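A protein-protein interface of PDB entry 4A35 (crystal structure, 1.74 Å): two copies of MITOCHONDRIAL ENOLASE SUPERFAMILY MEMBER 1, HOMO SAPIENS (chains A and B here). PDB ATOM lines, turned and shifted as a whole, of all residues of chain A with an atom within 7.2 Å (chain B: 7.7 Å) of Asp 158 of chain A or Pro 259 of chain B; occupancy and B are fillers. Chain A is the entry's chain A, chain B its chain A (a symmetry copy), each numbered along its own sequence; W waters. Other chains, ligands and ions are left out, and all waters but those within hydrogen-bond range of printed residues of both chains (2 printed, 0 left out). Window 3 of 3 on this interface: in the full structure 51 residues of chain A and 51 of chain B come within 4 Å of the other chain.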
ATOM      1  N   PHE A 153      11.191  16.482  18.409  1.00  0.00           N
ATOM      2  CA  PHE A 153      10.810  17.475  17.411  1.00  0.00           C
ATOM      3  C   PHE A 153      11.885  17.659  16.342  1.00  0.00           C
ATOM      4  O   PHE A 153      11.697  18.490  15.452  1.00  0.00           O
ATOM      5  CB  PHE A 153      10.484  18.833  18.051  1.00  0.00           C
ATOM      6  CG  PHE A 153       9.195  18.801  18.842  1.00  0.00           C
ATOM      7  CD1 PHE A 153       9.176  18.326  20.162  1.00  0.00           C
ATOM      8  CD2 PHE A 153       8.005  19.246  18.280  1.00  0.00           C
ATOM      9  CE1 PHE A 153       7.993  18.318  20.897  1.00  0.00           C
ATOM     10  CE2 PHE A 153       6.818  19.270  19.031  1.00  0.00           C
ATOM     11  CZ  PHE A 153       6.812  18.787  20.319  1.00  0.00           C
ATOM     12  N   ARG A 154      12.983  16.879  16.391  1.00  0.00           N
ATOM     13  CA  ARG A 154      13.996  17.048  15.342  1.00  0.00           C
ATOM     14  C   ARG A 154      13.366  16.930  13.937  1.00  0.00           C
ATOM     15  O   ARG A 154      12.548  16.045  13.693  1.00  0.00           O
ATOM     16  CB  ARG A 154      15.200  16.080  15.508  1.00  0.00           C
ATOM     17  CG  ARG A 154      16.281  16.347  14.455  1.00  0.00           C
ATOM     18  CD  ARG A 154      17.686  15.746  14.834  1.00  0.00           C
ATOM     19  NE  ARG A 154      17.640  14.279  14.829  1.00  0.00           N
ATOM     20  CZ  ARG A 154      18.688  13.484  15.076  1.00  0.00           C
ATOM     21  NH1 ARG A 154      19.863  14.008  15.438  1.00  0.00           N
ATOM     22  NH2 ARG A 154      18.547  12.155  15.040  1.00  0.00           N
ATOM     23  N   TYR A 155      13.774  17.817  13.031  1.00  0.00           N
ATOM     24  CA  TYR A 155      13.348  17.882  11.607  1.00  0.00           C
ATOM     25  C   TYR A 155      11.894  18.357  11.412  1.00  0.00           C
ATOM     26  O   TYR A 155      11.445  18.375  10.273  1.00  0.00           O
ATOM     27  CB  TYR A 155      13.548  16.567  10.869  1.00  0.00           C
ATOM     28  CG  TYR A 155      14.945  15.987  10.998  1.00  0.00           C
ATOM     29  CD1 TYR A 155      16.082  16.793  10.827  1.00  0.00           C
ATOM     30  CD2 TYR A 155      15.133  14.643  11.315  1.00  0.00           C
ATOM     31  CE1 TYR A 155      17.377  16.247  10.924  1.00  0.00           C
ATOM     32  CE2 TYR A 155      16.416  14.085  11.400  1.00  0.00           C
ATOM     33  CZ  TYR A 155      17.536  14.889  11.181  1.00  0.00           C
ATOM     34  OH  TYR A 155      18.812  14.341  11.272  1.00  0.00           O
ATOM     35  N   ILE A 156      11.165  18.712  12.498  1.00  0.00           N
ATOM     36  CA  ILE A 156       9.800  19.221  12.323  1.00  0.00           C
ATOM     37  C   ILE A 156       9.586  20.588  13.014  1.00  0.00           C
ATOM     38  O   ILE A 156       8.494  21.166  12.861  1.00  0.00           O
ATOM     39  CB  ILE A 156       8.667  18.221  12.747  1.00  0.00           C
ATOM     40  CG1 ILE A 156       8.623  18.003  14.302  1.00  0.00           C
ATOM     41  CG2 ILE A 156       8.768  16.885  11.964  1.00  0.00           C
ATOM     42  CD1 ILE A 156       7.391  17.175  14.857  1.00  0.00           C
ATOM     43  N   THR A 157      10.599  21.141  13.730  1.00  0.00           N
ATOM     44  CA  THR A 157      10.423  22.466  14.372  1.00  0.00           C
ATOM     45  C   THR A 157      10.123  23.601  13.362  1.00  0.00           C
ATOM     46  O   THR A 157       9.623  24.631  13.768  1.00  0.00           O
ATOM     47  CB  THR A 157      11.692  22.860  15.181  1.00  0.00           C
ATOM     48  OG1 THR A 157      12.800  22.950  14.271  1.00  0.00           O
ATOM     49  CG2 THR A 157      11.991  21.876  16.297  1.00  0.00           C
ATOM     50  N   ASP A 158      10.394  23.397  12.055  1.00  0.00           N
ATOM     51  CA  ASP A 158      10.091  24.373  11.003  1.00  0.00           C
ATOM     52  C   ASP A 158       8.563  24.464  10.728  1.00  0.00           C
ATOM     53  O   ASP A 158       8.135  25.424  10.100  1.00  0.00           O
ATOM     54  CB  ASP A 158      10.868  24.075   9.715  1.00  0.00           C
ATOM     55  CG  ASP A 158      10.751  22.633   9.205  1.00  0.00           C
ATOM     56  OD1 ASP A 158      10.864  21.676  10.044  1.00  0.00           O
ATOM     57  OD2 ASP A 158      10.545  22.451   7.978  1.00  0.00           O
ATOM     58  N   VAL A 159       7.760  23.454  11.174  1.00  0.00           N
ATOM     59  CA  VAL A 159       6.274  23.495  11.027  1.00  0.00           C
ATOM     60  C   VAL A 159       5.582  23.394  12.405  1.00  0.00           C
ATOM     61  O   VAL A 159       4.453  23.829  12.544  1.00  0.00           O
ATOM     62  CB  VAL A 159       5.696  22.432  10.047  1.00  0.00           C
ATOM     63  CG1 VAL A 159       6.315  22.546   8.666  1.00  0.00           C
ATOM     64  CG2 VAL A 159       5.793  20.986  10.592  1.00  0.00           C
ATOM     65  N   LEU A 160       6.251  22.811  13.395  1.00  0.00           N
ATOM     66  CA  LEU A 160       5.662  22.558  14.731  1.00  0.00           C
ATOM     67  C   LEU A 160       6.755  22.594  15.784  1.00  0.00           C
ATOM     68  O   LEU A 160       7.514  21.619  15.960  1.00  0.00           O
ATOM     69  CB  LEU A 160       4.929  21.184  14.742  1.00  0.00           C
ATOM     70  CG  LEU A 160       4.205  20.793  16.057  1.00  0.00           C
ATOM     71  CD1 LEU A 160       2.741  21.368  16.104  1.00  0.00           C
ATOM     72  CD2 LEU A 160       4.200  19.246  16.228  1.00  0.00           C
ATOM     73  N   THR A 161       6.850  23.746  16.469  1.00  0.00           N
ATOM     74  CA  THR A 161       7.774  23.886  17.594  1.00  0.00           C
ATOM     75  C   THR A 161       7.130  23.251  18.836  1.00  0.00           C
ATOM     76  O   THR A 161       5.932  22.905  18.823  1.00  0.00           O
ATOM     77  CB  THR A 161       8.078  25.383  17.861  1.00  0.00           C
ATOM     78  OG1 THR A 161       6.864  26.042  18.293  1.00  0.00           O
ATOM     79  CG2 THR A 161       8.681  26.115  16.632  1.00  0.00           C
ATOM     80  N   ASP A 164       4.335  25.486  19.771  1.00  0.00           N
ATOM     81  CA  ASP A 164       3.149  25.268  18.894  1.00  0.00           C
ATOM     82  C   ASP A 164       2.344  24.061  19.382  1.00  0.00           C
ATOM     83  O   ASP A 164       1.120  24.102  19.355  1.00  0.00           O
ATOM     84  CB  ASP A 164       3.535  24.970  17.437  1.00  0.00           C
ATOM     85  CG  ASP A 164       4.150  26.100  16.661  1.00  0.00           C
ATOM     86  OD1 ASP A 164       3.842  27.277  16.974  1.00  0.00           O
ATOM     87  OD2 ASP A 164       4.946  25.815  15.751  1.00  0.00           O
ATOM     88  N   LYS A 315       5.390  15.408   7.450  1.00  0.00           N
ATOM     89  CA  LYS A 315       5.550  16.861   7.436  1.00  0.00           C
ATOM     90  C   LYS A 315       5.479  17.400   6.015  1.00  0.00           C
ATOM     91  O   LYS A 315       4.739  18.338   5.750  1.00  0.00           O
ATOM     92  CB  LYS A 315       6.869  17.293   8.112  1.00  0.00           C
ATOM     93  CG  LYS A 315       7.164  18.806   7.914  1.00  0.00           C
ATOM     94  CD  LYS A 315       8.523  19.168   8.462  1.00  0.00           C
ATOM     95  CE  LYS A 315       9.695  18.781   7.526  1.00  0.00           C
ATOM     96  NZ  LYS A 315      10.917  19.605   7.838  1.00  0.00           N
ATOM     97  N   GLN A 319       3.002  19.926   4.169  1.00  0.00           N
ATOM     98  CA  GLN A 319       3.598  21.139   3.542  1.00  0.00           C
ATOM     99  C   GLN A 319       3.172  21.314   2.070  1.00  0.00           C
ATOM    100  O   GLN A 319       2.803  22.421   1.672  1.00  0.00           O
ATOM    101  CB  GLN A 319       5.107  21.119   3.624  1.00  0.00           C
ATOM    102  CG  GLN A 319       5.599  21.447   5.016  1.00  0.00           C
ATOM    103  CD  GLN A 319       7.095  21.286   5.120  1.00  0.00           C
ATOM    104  OE1 GLN A 319       7.666  20.296   4.668  1.00  0.00           O
ATOM    105  NE2 GLN A 319       7.765  22.309   5.649  1.00  0.00           N
ATOM    106  N   LYS A 348      -2.271  21.158  13.352  1.00  0.00           N
ATOM    107  CA  LYS A 348      -1.583  22.423  12.986  1.00  0.00           C
ATOM    108  C   LYS A 348      -1.912  22.793  11.513  1.00  0.00           C
ATOM    109  O   LYS A 348      -2.243  23.957  11.239  1.00  0.00           O
ATOM    110  CB  LYS A 348      -0.051  22.305  13.218  1.00  0.00           C
ATOM    111  CG  LYS A 348       0.744  23.594  12.898  1.00  0.00           C
ATOM    112  CD  LYS A 348       0.771  24.567  14.094  1.00  0.00           C
ATOM    113  CE  LYS A 348       1.202  25.993  13.769  1.00  0.00           C
ATOM    114  NZ  LYS A 348       2.561  26.053  13.231  1.00  0.00           N
ATOM    115  N   PHE A 349      -1.957  21.776  10.608  1.00  0.00           N
ATOM    116  CA  PHE A 349      -2.310  21.960   9.202  1.00  0.00           C
ATOM    117  C   PHE A 349      -3.833  21.801   8.932  1.00  0.00           C
ATOM    118  O   PHE A 349      -4.259  21.889   7.762  1.00  0.00           O
ATOM    119  CB  PHE A 349      -1.517  20.955   8.338  1.00  0.00           C
ATOM    120  CG  PHE A 349      -0.089  21.373   8.085  1.00  0.00           C
ATOM    121  CD1 PHE A 349       0.925  21.051   8.996  1.00  0.00           C
ATOM    122  CD2 PHE A 349       0.252  22.090   6.932  1.00  0.00           C
ATOM    123  CE1 PHE A 349       2.257  21.456   8.761  1.00  0.00           C
ATOM    124  CE2 PHE A 349       1.582  22.488   6.690  1.00  0.00           C
ATOM    125  CZ  PHE A 349       2.581  22.155   7.594  1.00  0.00           C
ATOM    126  N   TRP B 256      21.139  19.301  11.129  1.00  0.00           N
ATOM    127  CA  TRP B 256      20.328  20.482  11.380  1.00  0.00           C
ATOM    128  C   TRP B 256      18.884  20.428  10.971  1.00  0.00           C
ATOM    129  O   TRP B 256      18.513  19.644  10.087  1.00  0.00           O
ATOM    130  CB  TRP B 256      20.994  21.689  10.643  1.00  0.00           C
ATOM    131  CG  TRP B 256      22.465  21.909  10.944  1.00  0.00           C
ATOM    132  CD1 TRP B 256      23.060  21.941  12.177  1.00  0.00           C
ATOM    133  CD2 TRP B 256      23.505  22.220   9.988  1.00  0.00           C
ATOM    134  NE1 TRP B 256      24.419  22.203  12.043  1.00  0.00           N
ATOM    135  CE2 TRP B 256      24.697  22.453  10.719  1.00  0.00           C
ATOM    136  CE3 TRP B 256      23.538  22.356   8.584  1.00  0.00           C
ATOM    137  CZ2 TRP B 256      25.917  22.764  10.085  1.00  0.00           C
ATOM    138  CZ3 TRP B 256      24.713  22.782   7.973  1.00  0.00           C
ATOM    139  CH2 TRP B 256      25.902  22.936   8.713  1.00  0.00           C
ATOM    140  N   ASP B 257      18.045  21.244  11.672  1.00  0.00           N
ATOM    141  CA  ASP B 257      16.697  21.557  11.243  1.00  0.00           C
ATOM    142  C   ASP B 257      16.853  22.607  10.121  1.00  0.00           C
ATOM    143  O   ASP B 257      17.958  23.142   9.925  1.00  0.00           O
ATOM    144  CB  ASP B 257      15.801  22.035  12.413  1.00  0.00           C
ATOM    145  CG  ASP B 257      15.408  20.887  13.351  1.00  0.00           C
ATOM    146  OD1 ASP B 257      15.869  19.733  13.128  1.00  0.00           O
ATOM    147  OD2 ASP B 257      14.638  21.133  14.283  1.00  0.00           O
ATOM    148  N   VAL B 258      15.779  22.907   9.388  1.00  0.00           N
ATOM    149  CA  VAL B 258      15.899  23.742   8.195  1.00  0.00           C
ATOM    150  C   VAL B 258      16.385  25.189   8.539  1.00  0.00           C
ATOM    151  O   VAL B 258      17.408  25.608   7.989  1.00  0.00           O
ATOM    152  CB  VAL B 258      14.579  23.698   7.372  1.00  0.00           C
ATOM    153  CG1 VAL B 258      14.521  24.805   6.308  1.00  0.00           C
ATOM    154  CG2 VAL B 258      14.396  22.311   6.733  1.00  0.00           C
ATOM    155  N   PRO B 259      15.710  25.967   9.431  1.00  0.00           N
ATOM    156  CA  PRO B 259      16.210  27.325   9.721  1.00  0.00           C
ATOM    157  C   PRO B 259      17.621  27.284  10.328  1.00  0.00           C
ATOM    158  O   PRO B 259      18.466  28.109   9.959  1.00  0.00           O
ATOM    159  CB  PRO B 259      15.165  27.875  10.715  1.00  0.00           C
ATOM    160  CG  PRO B 259      13.928  27.072  10.417  1.00  0.00           C
ATOM    161  CD  PRO B 259      14.451  25.705  10.163  1.00  0.00           C
ATOM    162  N   GLU B 260      17.881  26.304  11.212  1.00  0.00           N
ATOM    163  CA  GLU B 260      19.196  26.121  11.842  1.00  0.00           C
ATOM    164  C   GLU B 260      20.305  25.919  10.797  1.00  0.00           C
ATOM    165  O   GLU B 260      21.379  26.509  10.955  1.00  0.00           O
ATOM    166  CB  GLU B 260      19.150  24.923  12.792  1.00  0.00           C
ATOM    167  CG  GLU B 260      20.479  24.558  13.423  1.00  0.00           C
ATOM    168  CD  GLU B 260      20.423  23.286  14.239  1.00  0.00           C
ATOM    169  OE1 GLU B 260      19.523  22.438  13.994  1.00  0.00           O
ATOM    170  OE2 GLU B 260      21.281  23.149  15.143  1.00  0.00           O
ATOM    171  N   ALA B 261      20.044  25.123   9.741  1.00  0.00           N
ATOM    172  CA  ALA B 261      21.049  24.888   8.683  1.00  0.00           C
ATOM    173  C   ALA B 261      21.421  26.209   7.995  1.00  0.00           C
ATOM    174  O   ALA B 261      22.594  26.469   7.734  1.00  0.00           O
ATOM    175  CB  ALA B 261      20.523  23.922   7.648  1.00  0.00           C
ATOM    176  N   VAL B 262      20.417  27.066   7.728  1.00  0.00           N
ATOM    177  CA  VAL B 262      20.690  28.342   7.078  1.00  0.00           C
ATOM    178  C   VAL B 262      21.512  29.232   7.982  1.00  0.00           C
ATOM    179  O   VAL B 262      22.470  29.857   7.528  1.00  0.00           O
ATOM    180  CB  VAL B 262      19.374  29.045   6.620  1.00  0.00           C
ATOM    181  CG1 VAL B 262      19.644  30.458   6.072  1.00  0.00           C
ATOM    182  CG2 VAL B 262      18.653  28.177   5.584  1.00  0.00           C
ATOM    183  N   GLU B 263      21.172  29.273   9.271  1.00  0.00           N
ATOM    184  CA  GLU B 263      21.896  30.141  10.200  1.00  0.00           C
ATOM    185  C   GLU B 263      23.383  29.714  10.389  1.00  0.00           C
ATOM    186  O   GLU B 263      24.305  30.550  10.352  1.00  0.00           O
ATOM    187  CB  GLU B 263      21.155  30.160  11.556  1.00  0.00           C
ATOM    188  CG  GLU B 263      21.826  31.021  12.629  1.00  0.00           C
ATOM    189  CD  GLU B 263      22.096  32.483  12.304  1.00  0.00           C
ATOM    190  OE1 GLU B 263      21.411  33.049  11.420  1.00  0.00           O
ATOM    191  OE2 GLU B 263      22.984  33.072  12.963  1.00  0.00           O
ATOM    192  N   TRP B 264      23.587  28.441  10.618  1.00  0.00           N
ATOM    193  CA  TRP B 264      24.917  27.862  10.809  1.00  0.00           C
ATOM    194  C   TRP B 264      25.797  28.106   9.559  1.00  0.00           C
ATOM    195  O   TRP B 264      26.938  28.582   9.668  1.00  0.00           O
ATOM    196  CB  TRP B 264      24.758  26.367  11.107  1.00  0.00           C
ATOM    197  CG  TRP B 264      25.939  25.752  11.781  1.00  0.00           C
ATOM    198  CD1 TRP B 264      27.189  25.567  11.244  1.00  0.00           C
ATOM    199  CD2 TRP B 264      25.909  24.991  12.995  1.00  0.00           C
ATOM    200  NE1 TRP B 264      27.949  24.789  12.075  1.00  0.00           N
ATOM    201  CE2 TRP B 264      27.195  24.425  13.166  1.00  0.00           C
ATOM    202  CE3 TRP B 264      24.937  24.785  13.997  1.00  0.00           C
ATOM    203  CZ2 TRP B 264      27.524  23.624  14.273  1.00  0.00           C
ATOM    204  CZ3 TRP B 264      25.286  24.029  15.122  1.00  0.00           C
ATOM    205  CH2 TRP B 264      26.559  23.442  15.233  1.00  0.00           C
ATOM    206  N   MET B 265      25.220  27.884   8.373  1.00  0.00           N
ATOM    207  CA  MET B 265      25.944  28.063   7.103  1.00  0.00           C
ATOM    208  C   MET B 265      26.253  29.529   6.813  1.00  0.00           C
ATOM    209  O   MET B 265      27.281  29.815   6.172  1.00  0.00           O
ATOM    210  CB  MET B 265      25.217  27.403   5.932  1.00  0.00           C
ATOM    211  CG  MET B 265      25.340  25.872   5.953  1.00  0.00           C
ATOM    212  SD  MET B 265      27.065  25.283   6.109  1.00  0.00           S
ATOM    213  CE  MET B 265      27.816  26.138   4.647  1.00  0.00           C
ATOM    214  N   THR B 280      20.342  18.593   6.289  1.00  0.00           N
ATOM    215  CA  THR B 280      19.248  18.151   7.153  1.00  0.00           C
ATOM    216  C   THR B 280      18.935  16.680   6.835  1.00  0.00           C
ATOM    217  O   THR B 280      19.733  16.018   6.117  1.00  0.00           O
ATOM    218  CB  THR B 280      18.022  19.098   7.014  1.00  0.00           C
ATOM    219  OG1 THR B 280      17.142  18.829   8.085  1.00  0.00           O
ATOM    220  CG2 THR B 280      17.269  18.960   5.637  1.00  0.00           C
ATOM    221  N   ASP B 284      14.202  14.818   3.770  1.00  0.00           N
ATOM    222  CA  ASP B 284      13.493  16.090   3.645  1.00  0.00           C
ATOM    223  C   ASP B 284      13.836  16.765   2.324  1.00  0.00           C
ATOM    224  O   ASP B 284      14.729  17.594   2.252  1.00  0.00           O
ATOM    225  CB  ASP B 284      13.831  16.983   4.833  1.00  0.00           C
ATOM    226  CG  ASP B 284      12.793  18.074   5.077  1.00  0.00           C
ATOM    227  OD1 ASP B 284      11.889  18.289   4.172  1.00  0.00           O
ATOM    228  OD2 ASP B 284      12.864  18.700   6.137  1.00  0.00           O
ATOM    229  N   LEU B 286      11.727  18.847   0.598  1.00  0.00           N
ATOM    230  CA  LEU B 286      11.312  20.246   0.670  1.00  0.00           C
ATOM    231  C   LEU B 286      12.303  21.053   1.514  1.00  0.00           C
ATOM    232  O   LEU B 286      12.576  22.229   1.172  1.00  0.00           O
ATOM    233  CB  LEU B 286       9.885  20.397   1.218  1.00  0.00           C
ATOM    234  CG  LEU B 286       8.754  19.598   0.447  1.00  0.00           C
ATOM    235  CD1 LEU B 286       7.360  19.925   1.050  1.00  0.00           C
ATOM    236  CD2 LEU B 286       8.762  19.911  -1.038  1.00  0.00           C
ATOM    237  N   GLY B 287      12.839  20.415   2.548  1.00  0.00           N
ATOM    238  CA  GLY B 287      13.841  21.039   3.413  1.00  0.00           C
ATOM    239  C   GLY B 287      15.128  21.392   2.693  1.00  0.00           C
ATOM    240  O   GLY B 287      15.665  22.507   2.848  1.00  0.00           O
ATOM    241  N   THR B 290      14.413  24.334   0.527  1.00  0.00           N
ATOM    242  CA  THR B 290      14.370  25.585   1.311  1.00  0.00           C
ATOM    243  C   THR B 290      15.813  26.104   1.609  1.00  0.00           C
ATOM    244  O   THR B 290      16.084  27.308   1.457  1.00  0.00           O
ATOM    245  CB  THR B 290      13.532  25.390   2.604  1.00  0.00           C
ATOM    246  OG1 THR B 290      12.212  25.061   2.222  1.00  0.00           O
ATOM    247  CG2 THR B 290      13.512  26.653   3.493  1.00  0.00           C
ATOM    248  N   ILE B 291      16.719  25.198   2.001  1.00  0.00           N
ATOM    249  CA  ILE B 291      18.105  25.550   2.347  1.00  0.00           C
ATOM    250  C   ILE B 291      18.825  25.980   1.067  1.00  0.00           C
ATOM    251  O   ILE B 291      19.514  26.991   1.077  1.00  0.00           O
ATOM    252  CB  ILE B 291      18.794  24.370   3.050  1.00  0.00           C
ATOM    253  CG1 ILE B 291      18.081  24.061   4.403  1.00  0.00           C
ATOM    254  CG2 ILE B 291      20.326  24.635   3.249  1.00  0.00           C
ATOM    255  CD1 ILE B 291      18.337  22.574   5.011  1.00  0.00           C
HETATM  256  O   HOH W   1      10.509  20.584   4.671  1.00  0.00           O
HETATM  257  O   HOH W   2      13.657  21.034   9.952  1.00  0.00           O
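N of Tyr 155 of chain A is in hydrogen-bond range of OD1 of Asp 257 of chain B (2.8 Å).
The side-chain hydroxyl (OG1) of Thr 157 of chain A lies within hydrogen-bond range of the side-chain carboxylate (OD2) of Asp 257 of chain B (2.6 Å).
NZ of Lys 315 of chain A is in salt-bridge range of OD2 of Asp 284 of chain B (2.7 Å).
The backbone carbonyl oxygen of Trp 256 of chain B is in hydrogen-bond range of the side-chain hydroxyl of Thr 280 of chain B, 2.6 Å away.
The side-chain carboxylate (OD1) of Asp 284 of chain B is in hydrogen-bond range of the backbone NH (N) of Gly 287 of chain B (2.8 Å).
The backbone carbonyl oxygen (O) of Tyr 155 of chain A is in hydrogen-bond range of the side-chain amino group (NZ) of Lys 315 of chain A (2.8 Å).
The backbone NH of Asp 257 of chain B is in hydrogen-bond range of the side-chain carboxylate of Glu 260 of chain B, at 3.0 Å.
The side-chain hydroxyl (OG1) of Thr 290 of chain B is in hydrogen-bond range of the backbone carbonyl oxygen (O) of Leu 286 of chain B (3.0 Å).
NZ of Lys 315 of chain A lies within salt-bridge range of OD2 of Asp 158 of chain A (2.9 Å).
Among the printed residues, pairs that only touch across the chains: Tyr 155 of chain A with Thr 280 of chain B, Gln 319 of chain A with Leu 286 of chain B, Arg 154 of chain A with Asp 257 of chain B, Tyr 155 of chain A with Trp 256 of chain B and Asp 158 of chain A with Pro 259 of chain B.
Of chain B, only Pro 259 comes within 4 Å of Asp 158 of chain A.
Pro 259 of chain B touches just one residue of chain A: Asp 158 (3.96 Å).
Printed residues of chain B within 4 Å of Tyr 155 of chain A: Trp 256, Asp 257 and Thr 280.
Of the printed residues of chain A, Thr 280 of chain B touches Tyr 155.
Of the printed residues of chain B, Lys 315 of chain A touches Asp 284 (2.7 Å).
Glu 260 of chain B touches none of the printed residues of chain A.
Phe 349 of chain A touches none of the printed residues of chain B.
The nearest residue of chain B that does not touch Asp 158 of chain A is Val 258 of chain B (4.05 Å).
The nearest residue of chain A that does not touch Pro 259 of chain B is Thr 157 of chain A (5.2 Å).
Of the 14 printed residues of chain A, 6 touch a printed residue of chain B.
Hydrophobic or aromatic side chains of chain A that line the printed part of chain B: Tyr 155.
Of the 16 printed residues of chain B, 6 touch a printed residue of chain A.
Hydrophobic or aromatic side chains of chain B within 4 Å of the printed part of chain A: Pro 259 and Leu 286.
Among the printed residues, 8 pairs touch across the chains.
Among the printed residues, Asp or Glu carboxylates within 4 Å of a Lys or Arg side-chain nitrogen of the other chain: Lys 315 of chain A with Asp 284 of chain B.
No position is printed for both chains.
Of the 8 pairs that touch across the chains among the printed residues, none has its exchanged pair printed and touching as well.
Water W1 lies within hydrogen-bond range of the side-chain carboxylate of Asp 284 of chain B, the side-chain amide oxygen of Gln 319 of chain A, the backbone NH of Gly 287 of chain B and the side-chain amino group of Lys 315 of chain A.
Water W2 lies within hydrogen-bond range of the side-chain carboxylate of Asp 158 of chain A (2.9 Å), the backbone NH of Val 258 of chain B (2.9 Å) and the backbone carbonyl oxygen of Tyr 155 of chain A (3.5 Å).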
